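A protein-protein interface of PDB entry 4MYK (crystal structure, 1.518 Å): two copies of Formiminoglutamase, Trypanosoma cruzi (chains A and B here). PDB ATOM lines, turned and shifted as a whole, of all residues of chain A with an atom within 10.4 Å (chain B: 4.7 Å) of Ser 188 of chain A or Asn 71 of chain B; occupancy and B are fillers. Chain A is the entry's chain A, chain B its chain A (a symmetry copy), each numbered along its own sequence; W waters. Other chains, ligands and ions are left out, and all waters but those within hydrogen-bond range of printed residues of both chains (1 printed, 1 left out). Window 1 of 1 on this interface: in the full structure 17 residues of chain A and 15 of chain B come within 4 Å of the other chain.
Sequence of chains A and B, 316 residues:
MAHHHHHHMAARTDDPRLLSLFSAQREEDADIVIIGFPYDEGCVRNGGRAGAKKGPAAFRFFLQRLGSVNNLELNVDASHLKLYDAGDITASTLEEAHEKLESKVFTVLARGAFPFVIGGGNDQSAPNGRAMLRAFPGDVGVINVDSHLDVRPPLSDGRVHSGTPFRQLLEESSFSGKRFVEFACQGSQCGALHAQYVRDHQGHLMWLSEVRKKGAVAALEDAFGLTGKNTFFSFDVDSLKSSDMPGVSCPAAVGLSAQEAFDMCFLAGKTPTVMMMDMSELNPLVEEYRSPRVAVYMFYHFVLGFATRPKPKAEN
Of chain B, only Gly 67, Ser 68, Asn 71, Tyr 297 and Tyr 300 come within 4 Å of Ser 188 of chain A. Asn 71 of chain B touches two residues of chain A. Gly 67 of chain B touches just one residue of chain A: Ser 188 (3.8 Å). No residue of chain A comes within 4 Å of Asn 70 of chain B. Of chain A, only Ala 192 and Trp 207 come within 4 Å of Leu 72 of chain B. No residue of chain A comes within 4 Å of Asn 75 of chain B. No residue of chain A comes within 4 Å of Val 76 of chain B. Printed residues of chain B within 4 Å of Ala 192 of chain A: Leu 72. Printed residues of chain B within 4 Å of Cys 185 of chain A: Glu 73. Ala 184 of chain A touches none of the printed residues of chain B. Asp 238 of chain A touches none of the printed residues of chain B. The nearest printed residue of chain B that does not touch Ser 188 of chain A is Glu 73 of chain B (4.8 Å). The nearest printed residue of chain A that does not touch Asn 71 of chain B is Cys 190 of chain A (5.8 Å). The nearest printed residue of chain A that does not touch Tyr 300 of chain B is Gln 189 of chain A (5.7 Å).
The side-chain amide nitrogen (ND2) of Asn 71 of chain B sits close to the backbone carbonyl oxygen (O) of Gly 187 of chain A. The backbone NH (N) of Gly 187 of chain A lies within hydrogen-bond range of the side-chain carboxylate (OE1) of Glu 73 of chain B (2.7 Å). The backbone carbonyl oxygen (O) of Ser 188 of chain A is in hydrogen-bond range of the backbone NH (N) of Ser 68 of chain B (3.3 Å). OG of Ser 209 of chain A lies within hydrogen-bond range of OE2 of Glu 73 of chain B (2.6 Å).
Water W1 lies within hydrogen-bond range of O of Ser 188 of chain A, OH of Tyr 297 of chain B and N of Gly 67 of chain B.
O of Ser 147 of chain A sits at hydrogen-bond distance from N of Gln 186 of chain A. NE2 of Gln 189 of chain A lies within hydrogen-bond range of NE2 of His 148 of chain A (3.0 Å). The backbone carbonyl oxygen of Gln 186 of chain A is in hydrogen-bond range of the side-chain sulfur of Cys 190 of chain A, at 3.2 Å. The backbone carbonyl oxygen (O) of Ser 68 of chain B is in hydrogen-bond range of the side-chain hydroxyl (OH) of Tyr 300 of chain B (2.6 Å).
No position is printed for both chains. Of the 18 pairs that touch across the chains among the printed residues, none has its exchanged pair printed and touching as well.
Hydrophobic or aromatic side chains of chain A that line the printed part of chain B: Ala 192 and Trp 207. Hydrophobic or aromatic side chains of chain B within 4 Å of the printed part of chain A: Leu 72, Tyr 297 and Tyr 300. Among the printed residues, 18 pairs touch across the chains. Among the printed residues, no Asp or Glu carboxylate lies within 4 Å of a Lys or Arg side-chain nitrogen of the other chain.
Gly 187 of chain A touches Tyr 300 of chain B (O to OH, 3.97 Å). Gly 67 of chain B touches Ser 188 of chain A (CA to O, 3.8 Å). N of Ser 188 of chain A touches ND2 of Asn 71 of chain B, at 3.5 Å. Ser 188 of chain A touches Tyr 297 of chain B. Gln 189 of chain A touches Tyr 297 of chain B (CG to OH, 3.6 Å). Leu 72 of chain B touches Ala 192 of chain A. Leu 72 of chain B touches Trp 207 of chain A (O to NE1, 3.7 Å).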
ATOM      1  N   ASP A 146      -7.733  -5.421 -27.580  1.00  0.00           N
ATOM      2  CA  ASP A 146      -9.069  -5.544 -27.042  1.00  0.00           C
ATOM      3  C   ASP A 146      -9.954  -4.513 -27.706  1.00  0.00           C
ATOM      4  O   ASP A 146      -9.570  -3.351 -27.816  1.00  0.00           O
ATOM      5  CB  ASP A 146      -9.009  -5.297 -25.539  1.00  0.00           C
ATOM      6  CG  ASP A 146     -10.238  -5.758 -24.826  1.00  0.00           C
ATOM      7  OD1 ASP A 146     -11.237  -6.085 -25.499  1.00  0.00           O
ATOM      8  OD2 ASP A 146     -10.194  -5.797 -23.585  1.00  0.00           O
ATOM      9  N   SER A 147     -11.130  -4.943 -28.165  1.00  0.00           N
ATOM     10  CA  SER A 147     -12.104  -4.023 -28.756  1.00  0.00           C
ATOM     11  C   SER A 147     -12.719  -3.175 -27.654  1.00  0.00           C
ATOM     12  O   SER A 147     -13.364  -2.162 -27.909  1.00  0.00           O
ATOM     13  CB  SER A 147     -13.189  -4.776 -29.533  1.00  0.00           C
ATOM     14  OG  SER A 147     -13.955  -5.626 -28.700  1.00  0.00           O
ATOM     15  N   HIS A 148     -12.503  -3.618 -26.421  1.00  0.00           N
ATOM     16  CA  HIS A 148     -13.031  -2.955 -25.241  1.00  0.00           C
ATOM     17  C   HIS A 148     -11.921  -2.209 -24.504  1.00  0.00           C
ATOM     18  O   HIS A 148     -10.751  -2.602 -24.515  1.00  0.00           O
ATOM     19  CB  HIS A 148     -13.719  -3.958 -24.296  1.00  0.00           C
ATOM     20  CG  HIS A 148     -14.831  -4.729 -24.938  1.00  0.00           C
ATOM     21  ND1 HIS A 148     -14.714  -6.056 -25.284  1.00  0.00           N
ATOM     22  CD2 HIS A 148     -16.078  -4.354 -25.312  1.00  0.00           C
ATOM     23  CE1 HIS A 148     -15.839  -6.469 -25.841  1.00  0.00           C
ATOM     24  NE2 HIS A 148     -16.684  -5.453 -25.874  1.00  0.00           N
ATOM     25  N   LEU A 149     -12.318  -1.107 -23.887  1.00  0.00           N
ATOM     26  CA  LEU A 149     -11.462  -0.340 -23.013  1.00  0.00           C
ATOM     27  C   LEU A 149     -12.286  -0.122 -21.749  1.00  0.00           C
ATOM     28  O   LEU A 149     -12.991   0.879 -21.613  1.00  0.00           O
ATOM     29  CB  LEU A 149     -11.066   0.968 -23.705  1.00  0.00           C
ATOM     30  CG  LEU A 149     -10.780   2.263 -22.950  1.00  0.00           C
ATOM     31  CD1 LEU A 149     -10.078   2.028 -21.613  1.00  0.00           C
ATOM     32  CD2 LEU A 149      -9.976   3.193 -23.858  1.00  0.00           C
ATOM     33  N   ALA A 184      -6.386  -1.554 -30.785  1.00  0.00           N
ATOM     34  CA  ALA A 184      -7.557  -1.955 -31.568  1.00  0.00           C
ATOM     35  C   ALA A 184      -8.849  -1.821 -30.780  1.00  0.00           C
ATOM     36  O   ALA A 184      -9.794  -2.576 -30.987  1.00  0.00           O
ATOM     37  CB  ALA A 184      -7.405  -3.376 -32.082  1.00  0.00           C
ATOM     38  N   CYS A 185      -8.880  -0.863 -29.865  1.00  0.00           N
ATOM     39  CA  CYS A 185     -10.105  -0.545 -29.156  1.00  0.00           C
ATOM     40  C   CYS A 185     -11.090   0.182 -30.087  1.00  0.00           C
ATOM     41  O   CYS A 185     -10.687   0.813 -31.068  1.00  0.00           O
ATOM     42  CB  CYS A 185      -9.798   0.278 -27.898  1.00  0.00           C
ATOM     43  SG  CYS A 185      -8.670   1.654 -28.181  1.00  0.00           S
ATOM     44  N   GLN A 186     -12.377   0.076 -29.768  1.00  0.00           N
ATOM     45  CA  GLN A 186     -13.443   0.575 -30.632  1.00  0.00           C
ATOM     46  C   GLN A 186     -14.245   1.717 -29.973  1.00  0.00           C
ATOM     47  O   GLN A 186     -14.828   1.523 -28.911  1.00  0.00           O
ATOM     48  CB  GLN A 186     -14.349  -0.586 -31.058  1.00  0.00           C
ATOM     49  CG  GLN A 186     -13.610  -1.574 -31.936  1.00  0.00           C
ATOM     50  CD  GLN A 186     -14.491  -2.681 -32.472  1.00  0.00           C
ATOM     51  OE1 GLN A 186     -15.697  -2.519 -32.614  1.00  0.00           O
ATOM     52  NE2 GLN A 186     -13.887  -3.818 -32.776  1.00  0.00           N
ATOM     53  N   GLY A 187     -14.263   2.895 -30.605  1.00  0.00           N
ATOM     54  CA  GLY A 187     -14.925   4.068 -30.049  1.00  0.00           C
ATOM     55  C   GLY A 187     -16.418   3.934 -29.755  1.00  0.00           C
ATOM     56  O   GLY A 187     -16.980   4.694 -28.967  1.00  0.00           O
ATOM     57  N   SER A 188     -17.062   2.960 -30.385  1.00  0.00           N
ATOM     58  CA  SER A 188     -18.481   2.685 -30.163  1.00  0.00           C
ATOM     59  C   SER A 188     -18.718   1.895 -28.882  1.00  0.00           C
ATOM     60  O   SER A 188     -19.861   1.688 -28.470  1.00  0.00           O
ATOM     61  CB  SER A 188     -19.024   1.880 -31.333  1.00  0.00           C
ATOM     62  OG  SER A 188     -18.131   0.822 -31.625  1.00  0.00           O
ATOM     63  N   GLN A 189     -17.624   1.454 -28.271  1.00  0.00           N
ATOM     64  CA  GLN A 189     -17.649   0.581 -27.104  1.00  0.00           C
ATOM     65  C   GLN A 189     -16.737   1.082 -25.999  1.00  0.00           C
ATOM     66  O   GLN A 189     -16.374   0.306 -25.117  1.00  0.00           O
ATOM     67  CB  GLN A 189     -17.138  -0.812 -27.478  1.00  0.00           C
ATOM     68  CG  GLN A 189     -18.079  -1.658 -28.282  1.00  0.00           C
ATOM     69  CD  GLN A 189     -17.829  -3.125 -28.039  1.00  0.00           C
ATOM     70  OE1 GLN A 189     -18.751  -3.876 -27.713  1.00  0.00           O
ATOM     71  NE2 GLN A 189     -16.566  -3.541 -28.167  1.00  0.00           N
ATOM     72  N   CYS A 190     -16.335   2.348 -26.048  1.00  0.00           N
ATOM     73  CA  CYS A 190     -15.430   2.855 -25.029  1.00  0.00           C
ATOM     74  C   CYS A 190     -15.918   4.140 -24.351  1.00  0.00           C
ATOM     75  O   CYS A 190     -16.021   5.200 -24.972  1.00  0.00           O
ATOM     76  CB  CYS A 190     -14.004   2.975 -25.581  1.00  0.00           C
ATOM     77  SG  CYS A 190     -13.299   1.346 -26.054  1.00  0.00           S
ATOM     78  N   GLY A 191     -16.231   4.020 -23.060  1.00  0.00           N
ATOM     79  CA  GLY A 191     -16.692   5.155 -22.283  1.00  0.00           C
ATOM     80  C   GLY A 191     -15.653   6.252 -22.384  1.00  0.00           C
ATOM     81  O   GLY A 191     -14.460   5.959 -22.471  1.00  0.00           O
ATOM     82  N   ALA A 192     -16.082   7.511 -22.396  1.00  0.00           N
ATOM     83  CA  ALA A 192     -15.120   8.609 -22.450  1.00  0.00           C
ATOM     84  C   ALA A 192     -14.369   8.822 -21.114  1.00  0.00           C
ATOM     85  O   ALA A 192     -13.205   9.243 -21.118  1.00  0.00           O
ATOM     86  CB  ALA A 192     -15.785   9.889 -22.929  1.00  0.00           C
ATOM     87  N   LEU A 193     -15.030   8.525 -19.990  1.00  0.00           N
ATOM     88  CA  LEU A 193     -14.372   8.481 -18.685  1.00  0.00           C
ATOM     89  C   LEU A 193     -13.273   7.418 -18.690  1.00  0.00           C
ATOM     90  O   LEU A 193     -12.226   7.582 -18.058  1.00  0.00           O
ATOM     91  CB  LEU A 193     -15.376   8.164 -17.569  1.00  0.00           C
ATOM     92  CG  LEU A 193     -16.347   9.246 -17.065  1.00  0.00           C
ATOM     93  CD1 LEU A 193     -17.237   8.712 -15.942  1.00  0.00           C
ATOM     94  CD2 LEU A 193     -15.599  10.481 -16.592  1.00  0.00           C
ATOM     95  N   HIS A 194     -13.532   6.321 -19.398  1.00  0.00           N
ATOM     96  CA  HIS A 194     -12.576   5.228 -19.527  1.00  0.00           C
ATOM     97  C   HIS A 194     -11.342   5.690 -20.297  1.00  0.00           C
ATOM     98  O   HIS A 194     -10.226   5.442 -19.880  1.00  0.00           O
ATOM     99  CB  HIS A 194     -13.221   4.010 -20.209  1.00  0.00           C
ATOM    100  CG  HIS A 194     -14.206   3.266 -19.347  1.00  0.00           C
ATOM    101  ND1 HIS A 194     -15.564   3.511 -19.377  1.00  0.00           N
ATOM    102  CD2 HIS A 194     -14.028   2.268 -18.449  1.00  0.00           C
ATOM    103  CE1 HIS A 194     -16.177   2.707 -18.527  1.00  0.00           C
ATOM    104  NE2 HIS A 194     -15.268   1.941 -17.952  1.00  0.00           N
ATOM    105  N   ALA A 195     -11.551   6.370 -21.420  1.00  0.00           N
ATOM    106  CA  ALA A 195     -10.445   6.941 -22.190  1.00  0.00           C
ATOM    107  C   ALA A 195      -9.681   7.952 -21.349  1.00  0.00           C
ATOM    108  O   ALA A 195      -8.463   7.869 -21.204  1.00  0.00           O
ATOM    109  CB  ALA A 195     -10.964   7.603 -23.460  1.00  0.00           C
ATOM    110  N   ARG A 199      -5.605   7.992 -20.541  1.00  0.00           N
ATOM    111  CA  ARG A 199      -4.812   9.099 -21.039  1.00  0.00           C
ATOM    112  C   ARG A 199      -4.286   9.956 -19.908  1.00  0.00           C
ATOM    113  O   ARG A 199      -3.156  10.435 -19.972  1.00  0.00           O
ATOM    114  CB  ARG A 199      -5.593   9.902 -22.073  1.00  0.00           C
ATOM    115  CG  ARG A 199      -5.555   9.226 -23.443  1.00  0.00           C
ATOM    116  CD  ARG A 199      -6.707   9.642 -24.325  1.00  0.00           C
ATOM    117  NE  ARG A 199      -6.519   9.198 -25.702  1.00  0.00           N
ATOM    118  CZ  ARG A 199      -7.377   9.435 -26.695  1.00  0.00           C
ATOM    119  NH1 ARG A 199      -8.500  10.114 -26.463  1.00  0.00           N
ATOM    120  NH2 ARG A 199      -7.111   8.990 -27.921  1.00  0.00           N
ATOM    121  N   LEU A 205      -4.061   5.234 -26.597  1.00  0.00           N
ATOM    122  CA  LEU A 205      -5.179   4.624 -27.300  1.00  0.00           C
ATOM    123  C   LEU A 205      -4.854   4.481 -28.772  1.00  0.00           C
ATOM    124  O   LEU A 205      -4.596   5.467 -29.453  1.00  0.00           O
ATOM    125  CB  LEU A 205      -6.447   5.457 -27.134  1.00  0.00           C
ATOM    126  CG  LEU A 205      -6.823   5.846 -25.704  1.00  0.00           C
ATOM    127  CD1 LEU A 205      -8.231   6.439 -25.684  1.00  0.00           C
ATOM    128  CD2 LEU A 205      -6.739   4.657 -24.778  1.00  0.00           C
ATOM    129  N   TRP A 207      -6.865   3.195 -31.649  1.00  0.00           N
ATOM    130  CA  TRP A 207      -8.191   2.788 -32.122  1.00  0.00           C
ATOM    131  C   TRP A 207      -8.090   1.862 -33.312  1.00  0.00           C
ATOM    132  O   TRP A 207      -7.152   1.961 -34.097  1.00  0.00           O
ATOM    133  CB  TRP A 207      -9.029   4.006 -32.517  1.00  0.00           C
ATOM    134  CG  TRP A 207      -9.250   4.986 -31.415  1.00  0.00           C
ATOM    135  CD1 TRP A 207      -8.673   6.208 -31.286  1.00  0.00           C
ATOM    136  CD2 TRP A 207     -10.106   4.823 -30.270  1.00  0.00           C
ATOM    137  NE1 TRP A 207      -9.117   6.823 -30.141  1.00  0.00           N
ATOM    138  CE2 TRP A 207      -9.999   5.992 -29.501  1.00  0.00           C
ATOM    139  CE3 TRP A 207     -10.953   3.797 -29.822  1.00  0.00           C
ATOM    140  CZ2 TRP A 207     -10.705   6.169 -28.309  1.00  0.00           C
ATOM    141  CZ3 TRP A 207     -11.655   3.980 -28.637  1.00  0.00           C
ATOM    142  CH2 TRP A 207     -11.528   5.153 -27.899  1.00  0.00           C
ATOM    143  N   LEU A 208      -9.056   0.956 -33.433  1.00  0.00           N
ATOM    144  CA  LEU A 208      -9.108   0.025 -34.559  1.00  0.00           C
ATOM    145  C   LEU A 208      -8.828   0.728 -35.902  1.00  0.00           C
ATOM    146  O   LEU A 208      -7.962   0.303 -36.666  1.00  0.00           O
ATOM    147  CB  LEU A 208     -10.468  -0.688 -34.586  1.00  0.00           C
ATOM    148  CG  LEU A 208     -10.720  -1.714 -35.694  1.00  0.00           C
ATOM    149  CD1 LEU A 208      -9.685  -2.826 -35.659  1.00  0.00           C
ATOM    150  CD2 LEU A 208     -12.120  -2.275 -35.602  1.00  0.00           C
ATOM    151  N   SER A 209      -9.551   1.818 -36.158  1.00  0.00           N
ATOM    152  CA  SER A 209      -9.440   2.558 -37.407  1.00  0.00           C
ATOM    153  C   SER A 209      -7.997   2.953 -37.742  1.00  0.00           C
ATOM    154  O   SER A 209      -7.594   2.947 -38.901  1.00  0.00           O
ATOM    155  CB  SER A 209     -10.364   3.787 -37.396  1.00  0.00           C
ATOM    156  OG  SER A 209     -10.062   4.659 -36.324  1.00  0.00           O
ATOM    157  N   ASP A 238     -11.843 -11.146 -28.548  1.00  0.00           N
ATOM    158  CA  ASP A 238     -13.046 -10.439 -28.987  1.00  0.00           C
ATOM    159  C   ASP A 238     -12.687  -9.106 -29.657  1.00  0.00           C
ATOM    160  O   ASP A 238     -13.561  -8.284 -29.957  1.00  0.00           O
ATOM    161  CB  ASP A 238     -14.072 -10.282 -27.854  1.00  0.00           C
ATOM    162  CG  ASP A 238     -13.707  -9.197 -26.851  1.00  0.00           C
ATOM    163  OD1 ASP A 238     -12.875  -8.313 -27.170  1.00  0.00           O
ATOM    164  OD2 ASP A 238     -14.276  -9.221 -25.734  1.00  0.00           O
ATOM    165  N   PRO A 251     -19.018 -10.963 -28.805  1.00  0.00           N
ATOM    166  CA  PRO A 251     -18.751 -10.961 -30.251  1.00  0.00           C
ATOM    167  C   PRO A 251     -18.678  -9.555 -30.872  1.00  0.00           C
ATOM    168  O   PRO A 251     -19.532  -8.687 -30.607  1.00  0.00           O
ATOM    169  CB  PRO A 251     -19.925 -11.767 -30.823  1.00  0.00           C
ATOM    170  CG  PRO A 251     -20.334 -12.679 -29.695  1.00  0.00           C
ATOM    171  CD  PRO A 251     -20.130 -11.869 -28.447  1.00  0.00           C
ATOM    172  N   ALA A 252     -17.648  -9.343 -31.692  1.00  0.00           N
ATOM    173  CA  ALA A 252     -17.399  -8.037 -32.287  1.00  0.00           C
ATOM    174  C   ALA A 252     -17.997  -7.945 -33.679  1.00  0.00           C
ATOM    175  O   ALA A 252     -17.829  -8.862 -34.491  1.00  0.00           O
ATOM    176  CB  ALA A 252     -15.901  -7.755 -32.338  1.00  0.00           C
ATOM    177  N   ALA A 253     -18.684  -6.836 -33.956  1.00  0.00           N
ATOM    178  CA  ALA A 253     -19.210  -6.595 -35.291  1.00  0.00           C
ATOM    179  C   ALA A 253     -18.076  -6.280 -36.262  1.00  0.00           C
ATOM    180  O   ALA A 253     -17.982  -6.886 -37.333  1.00  0.00           O
ATOM    181  CB  ALA A 253     -20.241  -5.484 -35.275  1.00  0.00           C
ATOM    182  N   VAL A 254     -17.229  -5.324 -35.887  1.00  0.00           N
ATOM    183  CA  VAL A 254     -15.997  -5.051 -36.624  1.00  0.00           C
ATOM    184  C   VAL A 254     -14.797  -5.381 -35.739  1.00  0.00           C
ATOM    185  O   VAL A 254     -14.946  -5.607 -34.530  1.00  0.00           O
ATOM    186  CB  VAL A 254     -15.894  -3.584 -37.108  1.00  0.00           C
ATOM    187  CG1 VAL A 254     -16.877  -3.311 -38.223  1.00  0.00           C
ATOM    188  CG2 VAL A 254     -16.109  -2.617 -35.959  1.00  0.00           C
ATOM    189  N   GLY A 255     -13.613  -5.403 -36.350  1.00  0.00           N
ATOM    190  CA  GLY A 255     -12.394  -5.711 -35.632  1.00  0.00           C
ATOM    191  C   GLY A 255     -11.358  -6.423 -36.482  1.00  0.00           C
ATOM    192  O   GLY A 255     -11.480  -6.515 -37.703  1.00  0.00           O
ATOM    193  N   GLY B  67     -23.783   1.640 -28.124  1.00  0.00           N
ATOM    194  CA  GLY B  67     -23.437   2.915 -28.736  1.00  0.00           C
ATOM    195  C   GLY B  67     -23.069   4.074 -27.826  1.00  0.00           C
ATOM    196  O   GLY B  67     -23.927   4.866 -27.466  1.00  0.00           O
ATOM    197  N   SER B  68     -21.795   4.202 -27.481  1.00  0.00           N
ATOM    198  CA  SER B  68     -21.364   5.324 -26.661  1.00  0.00           C
ATOM    199  C   SER B  68     -21.714   6.662 -27.313  1.00  0.00           C
ATOM    200  O   SER B  68     -21.285   6.939 -28.433  1.00  0.00           O
ATOM    201  CB  SER B  68     -19.858   5.240 -26.389  1.00  0.00           C
ATOM    202  OG  SER B  68     -19.527   4.028 -25.732  1.00  0.00           O
ATOM    203  N   VAL B  69     -22.496   7.490 -26.613  1.00  0.00           N
ATOM    204  CA  VAL B  69     -22.906   8.801 -27.139  1.00  0.00           C
ATOM    205  C   VAL B  69     -21.719   9.713 -27.464  1.00  0.00           C
ATOM    206  O   VAL B  69     -21.758  10.474 -28.432  1.00  0.00           O
ATOM    207  CB  VAL B  69     -23.885   9.529 -26.197  1.00  0.00           C
ATOM    208  CG1 VAL B  69     -25.090   8.650 -25.926  1.00  0.00           C
ATOM    209  CG2 VAL B  69     -23.205   9.902 -24.896  1.00  0.00           C
ATOM    210  N   ASN B  70     -20.659   9.637 -26.665  1.00  0.00           N
ATOM    211  CA  ASN B  70     -19.427  10.309 -27.048  1.00  0.00           C
ATOM    212  C   ASN B  70     -18.412   9.314 -27.558  1.00  0.00           C
ATOM    213  O   ASN B  70     -17.925   8.468 -26.807  1.00  0.00           O
ATOM    214  CB  ASN B  70     -18.841  11.111 -25.898  1.00  0.00           C
ATOM    215  CG  ASN B  70     -17.767  12.084 -26.356  1.00  0.00           C
ATOM    216  OD1 ASN B  70     -17.501  12.231 -27.552  1.00  0.00           O
ATOM    217  ND2 ASN B  70     -17.148  12.760 -25.397  1.00  0.00           N
ATOM    218  N   ASN B  71     -18.120   9.415 -28.850  1.00  0.00           N
ATOM    219  CA  ASN B  71     -17.215   8.507 -29.522  1.00  0.00           C
ATOM    220  C   ASN B  71     -15.897   9.220 -29.758  1.00  0.00           C
ATOM    221  O   ASN B  71     -15.817  10.157 -30.552  1.00  0.00           O
ATOM    222  CB  ASN B  71     -17.822   8.058 -30.851  1.00  0.00           C
ATOM    223  CG  ASN B  71     -16.953   7.048 -31.583  1.00  0.00           C
ATOM    224  OD1 ASN B  71     -15.743   7.219 -31.705  1.00  0.00           O
ATOM    225  ND2 ASN B  71     -17.574   5.987 -32.082  1.00  0.00           N
ATOM    226  N   LEU B  72     -14.858   8.773 -29.070  1.00  0.00           N
ATOM    227  CA  LEU B  72     -13.587   9.475 -29.123  1.00  0.00           C
ATOM    228  C   LEU B  72     -12.689   8.973 -30.221  1.00  0.00           C
ATOM    229  O   LEU B  72     -11.608   9.511 -30.443  1.00  0.00           O
ATOM    230  CB  LEU B  72     -12.882   9.402 -27.783  1.00  0.00           C
ATOM    231  CG  LEU B  72     -13.408  10.505 -26.869  1.00  0.00           C
ATOM    232  CD1 LEU B  72     -13.555   9.993 -25.453  1.00  0.00           C
ATOM    233  CD2 LEU B  72     -12.519  11.751 -26.953  1.00  0.00           C
ATOM    234  N   GLU B  73     -13.135   7.938 -30.910  1.00  0.00           N
ATOM    235  CA  GLU B  73     -12.417   7.477 -32.083  1.00  0.00           C
ATOM    236  C   GLU B  73     -12.793   8.332 -33.282  1.00  0.00           C
ATOM    237  O   GLU B  73     -11.940   8.690 -34.086  1.00  0.00           O
ATOM    238  CB  GLU B  73     -12.727   6.012 -32.359  1.00  0.00           C
ATOM    239  CG  GLU B  73     -11.899   5.435 -33.475  1.00  0.00           C
ATOM    240  CD  GLU B  73     -12.264   4.014 -33.764  1.00  0.00           C
ATOM    241  OE1 GLU B  73     -13.033   3.419 -32.981  1.00  0.00           O
ATOM    242  OE2 GLU B  73     -11.780   3.489 -34.775  1.00  0.00           O
ATOM    243  N   LEU B  74     -14.079   8.653 -33.394  1.00  0.00           N
ATOM    244  CA  LEU B  74     -14.564   9.556 -34.430  1.00  0.00           C
ATOM    245  C   LEU B  74     -14.567  10.981 -33.903  1.00  0.00           C
ATOM    246  O   LEU B  74     -14.697  11.931 -34.666  1.00  0.00           O
ATOM    247  CB  LEU B  74     -15.976   9.173 -34.852  1.00  0.00           C
ATOM    248  CG  LEU B  74     -16.144   7.696 -35.227  1.00  0.00           C
ATOM    249  CD1 LEU B  74     -17.506   7.478 -35.873  1.00  0.00           C
ATOM    250  CD2 LEU B  74     -14.998   7.209 -36.132  1.00  0.00           C
ATOM    251  N   ASN B  75     -14.412  11.107 -32.588  1.00  0.00           N
ATOM    252  CA  ASN B  75     -14.464  12.396 -31.901  1.00  0.00           C
ATOM    253  C   ASN B  75     -15.723  13.171 -32.242  1.00  0.00           C
ATOM    254  O   ASN B  75     -15.672  14.312 -32.692  1.00  0.00           O
ATOM    255  CB  ASN B  75     -13.197  13.225 -32.144  1.00  0.00           C
ATOM    256  CG  ASN B  75     -12.008  12.719 -31.332  1.00  0.00           C
ATOM    257  OD1 ASN B  75     -12.089  12.581 -30.105  1.00  0.00           O
ATOM    258  ND2 ASN B  75     -10.904  12.425 -32.015  1.00  0.00           N
ATOM    259  N   VAL B  76     -16.855  12.511 -32.032  1.00  0.00           N
ATOM    260  CA  VAL B  76     -18.163  13.133 -32.173  1.00  0.00           C
ATOM    261  C   VAL B  76     -18.971  12.853 -30.909  1.00  0.00           C
ATOM    262  O   VAL B  76     -19.095  11.703 -30.484  1.00  0.00           O
ATOM    263  CB  VAL B  76     -18.923  12.604 -33.423  1.00  0.00           C
ATOM    264  CG1 VAL B  76     -20.354  13.087 -33.426  1.00  0.00           C
ATOM    265  CG2 VAL B  76     -18.223  13.045 -34.697  1.00  0.00           C
ATOM    266  N   TYR B 297     -25.763  -0.658 -34.619  1.00  0.00           N
ATOM    267  CA  TYR B 297     -24.518   0.074 -34.821  1.00  0.00           C
ATOM    268  C   TYR B 297     -24.557   0.949 -36.068  1.00  0.00           C
ATOM    269  O   TYR B 297     -23.963   2.019 -36.109  1.00  0.00           O
ATOM    270  CB  TYR B 297     -23.327  -0.880 -34.873  1.00  0.00           C
ATOM    271  CG  TYR B 297     -22.793  -1.253 -33.502  1.00  0.00           C
ATOM    272  CD1 TYR B 297     -22.496  -0.269 -32.565  1.00  0.00           C
ATOM    273  CD2 TYR B 297     -22.575  -2.579 -33.151  1.00  0.00           C
ATOM    274  CE1 TYR B 297     -22.011  -0.599 -31.313  1.00  0.00           C
ATOM    275  CE2 TYR B 297     -22.084  -2.916 -31.903  1.00  0.00           C
ATOM    276  CZ  TYR B 297     -21.805  -1.923 -30.986  1.00  0.00           C
ATOM    277  OH  TYR B 297     -21.310  -2.246 -29.740  1.00  0.00           O
ATOM    278  N   TYR B 300     -26.589   3.832 -34.973  1.00  0.00           N
ATOM    279  CA  TYR B 300     -25.672   4.538 -34.096  1.00  0.00           C
ATOM    280  C   TYR B 300     -24.750   5.485 -34.872  1.00  0.00           C
ATOM    281  O   TYR B 300     -24.579   6.640 -34.497  1.00  0.00           O
ATOM    282  CB  TYR B 300     -24.849   3.521 -33.295  1.00  0.00           C
ATOM    283  CG  TYR B 300     -23.657   4.121 -32.588  1.00  0.00           C
ATOM    284  CD1 TYR B 300     -23.828   4.973 -31.506  1.00  0.00           C
ATOM    285  CD2 TYR B 300     -22.365   3.844 -33.004  1.00  0.00           C
ATOM    286  CE1 TYR B 300     -22.747   5.536 -30.858  1.00  0.00           C
ATOM    287  CE2 TYR B 300     -21.276   4.407 -32.370  1.00  0.00           C
ATOM    288  CZ  TYR B 300     -21.473   5.253 -31.293  1.00  0.00           C
ATOM    289  OH  TYR B 300     -20.395   5.817 -30.643  1.00  0.00           O
ATOM    290  N   LEU B 304     -24.513   9.594 -34.869  1.00  0.00           N
ATOM    291  CA  LEU B 304     -23.284  10.364 -34.720  1.00  0.00           C
ATOM    292  C   LEU B 304     -23.097  11.370 -35.855  1.00  0.00           C
ATOM    293  O   LEU B 304     -22.703  12.509 -35.622  1.00  0.00           O
ATOM    294  CB  LEU B 304     -22.077   9.435 -34.682  1.00  0.00           C
ATOM    295  CG  LEU B 304     -21.828   8.663 -33.391  1.00  0.00           C
ATOM    296  CD1 LEU B 304     -20.554   7.865 -33.523  1.00  0.00           C
ATOM    297  CD2 LEU B 304     -21.733   9.613 -32.220  1.00  0.00           C
HETATM  298  O   HOH W   1     -21.695  -0.278 -27.764  1.00  0.00           O
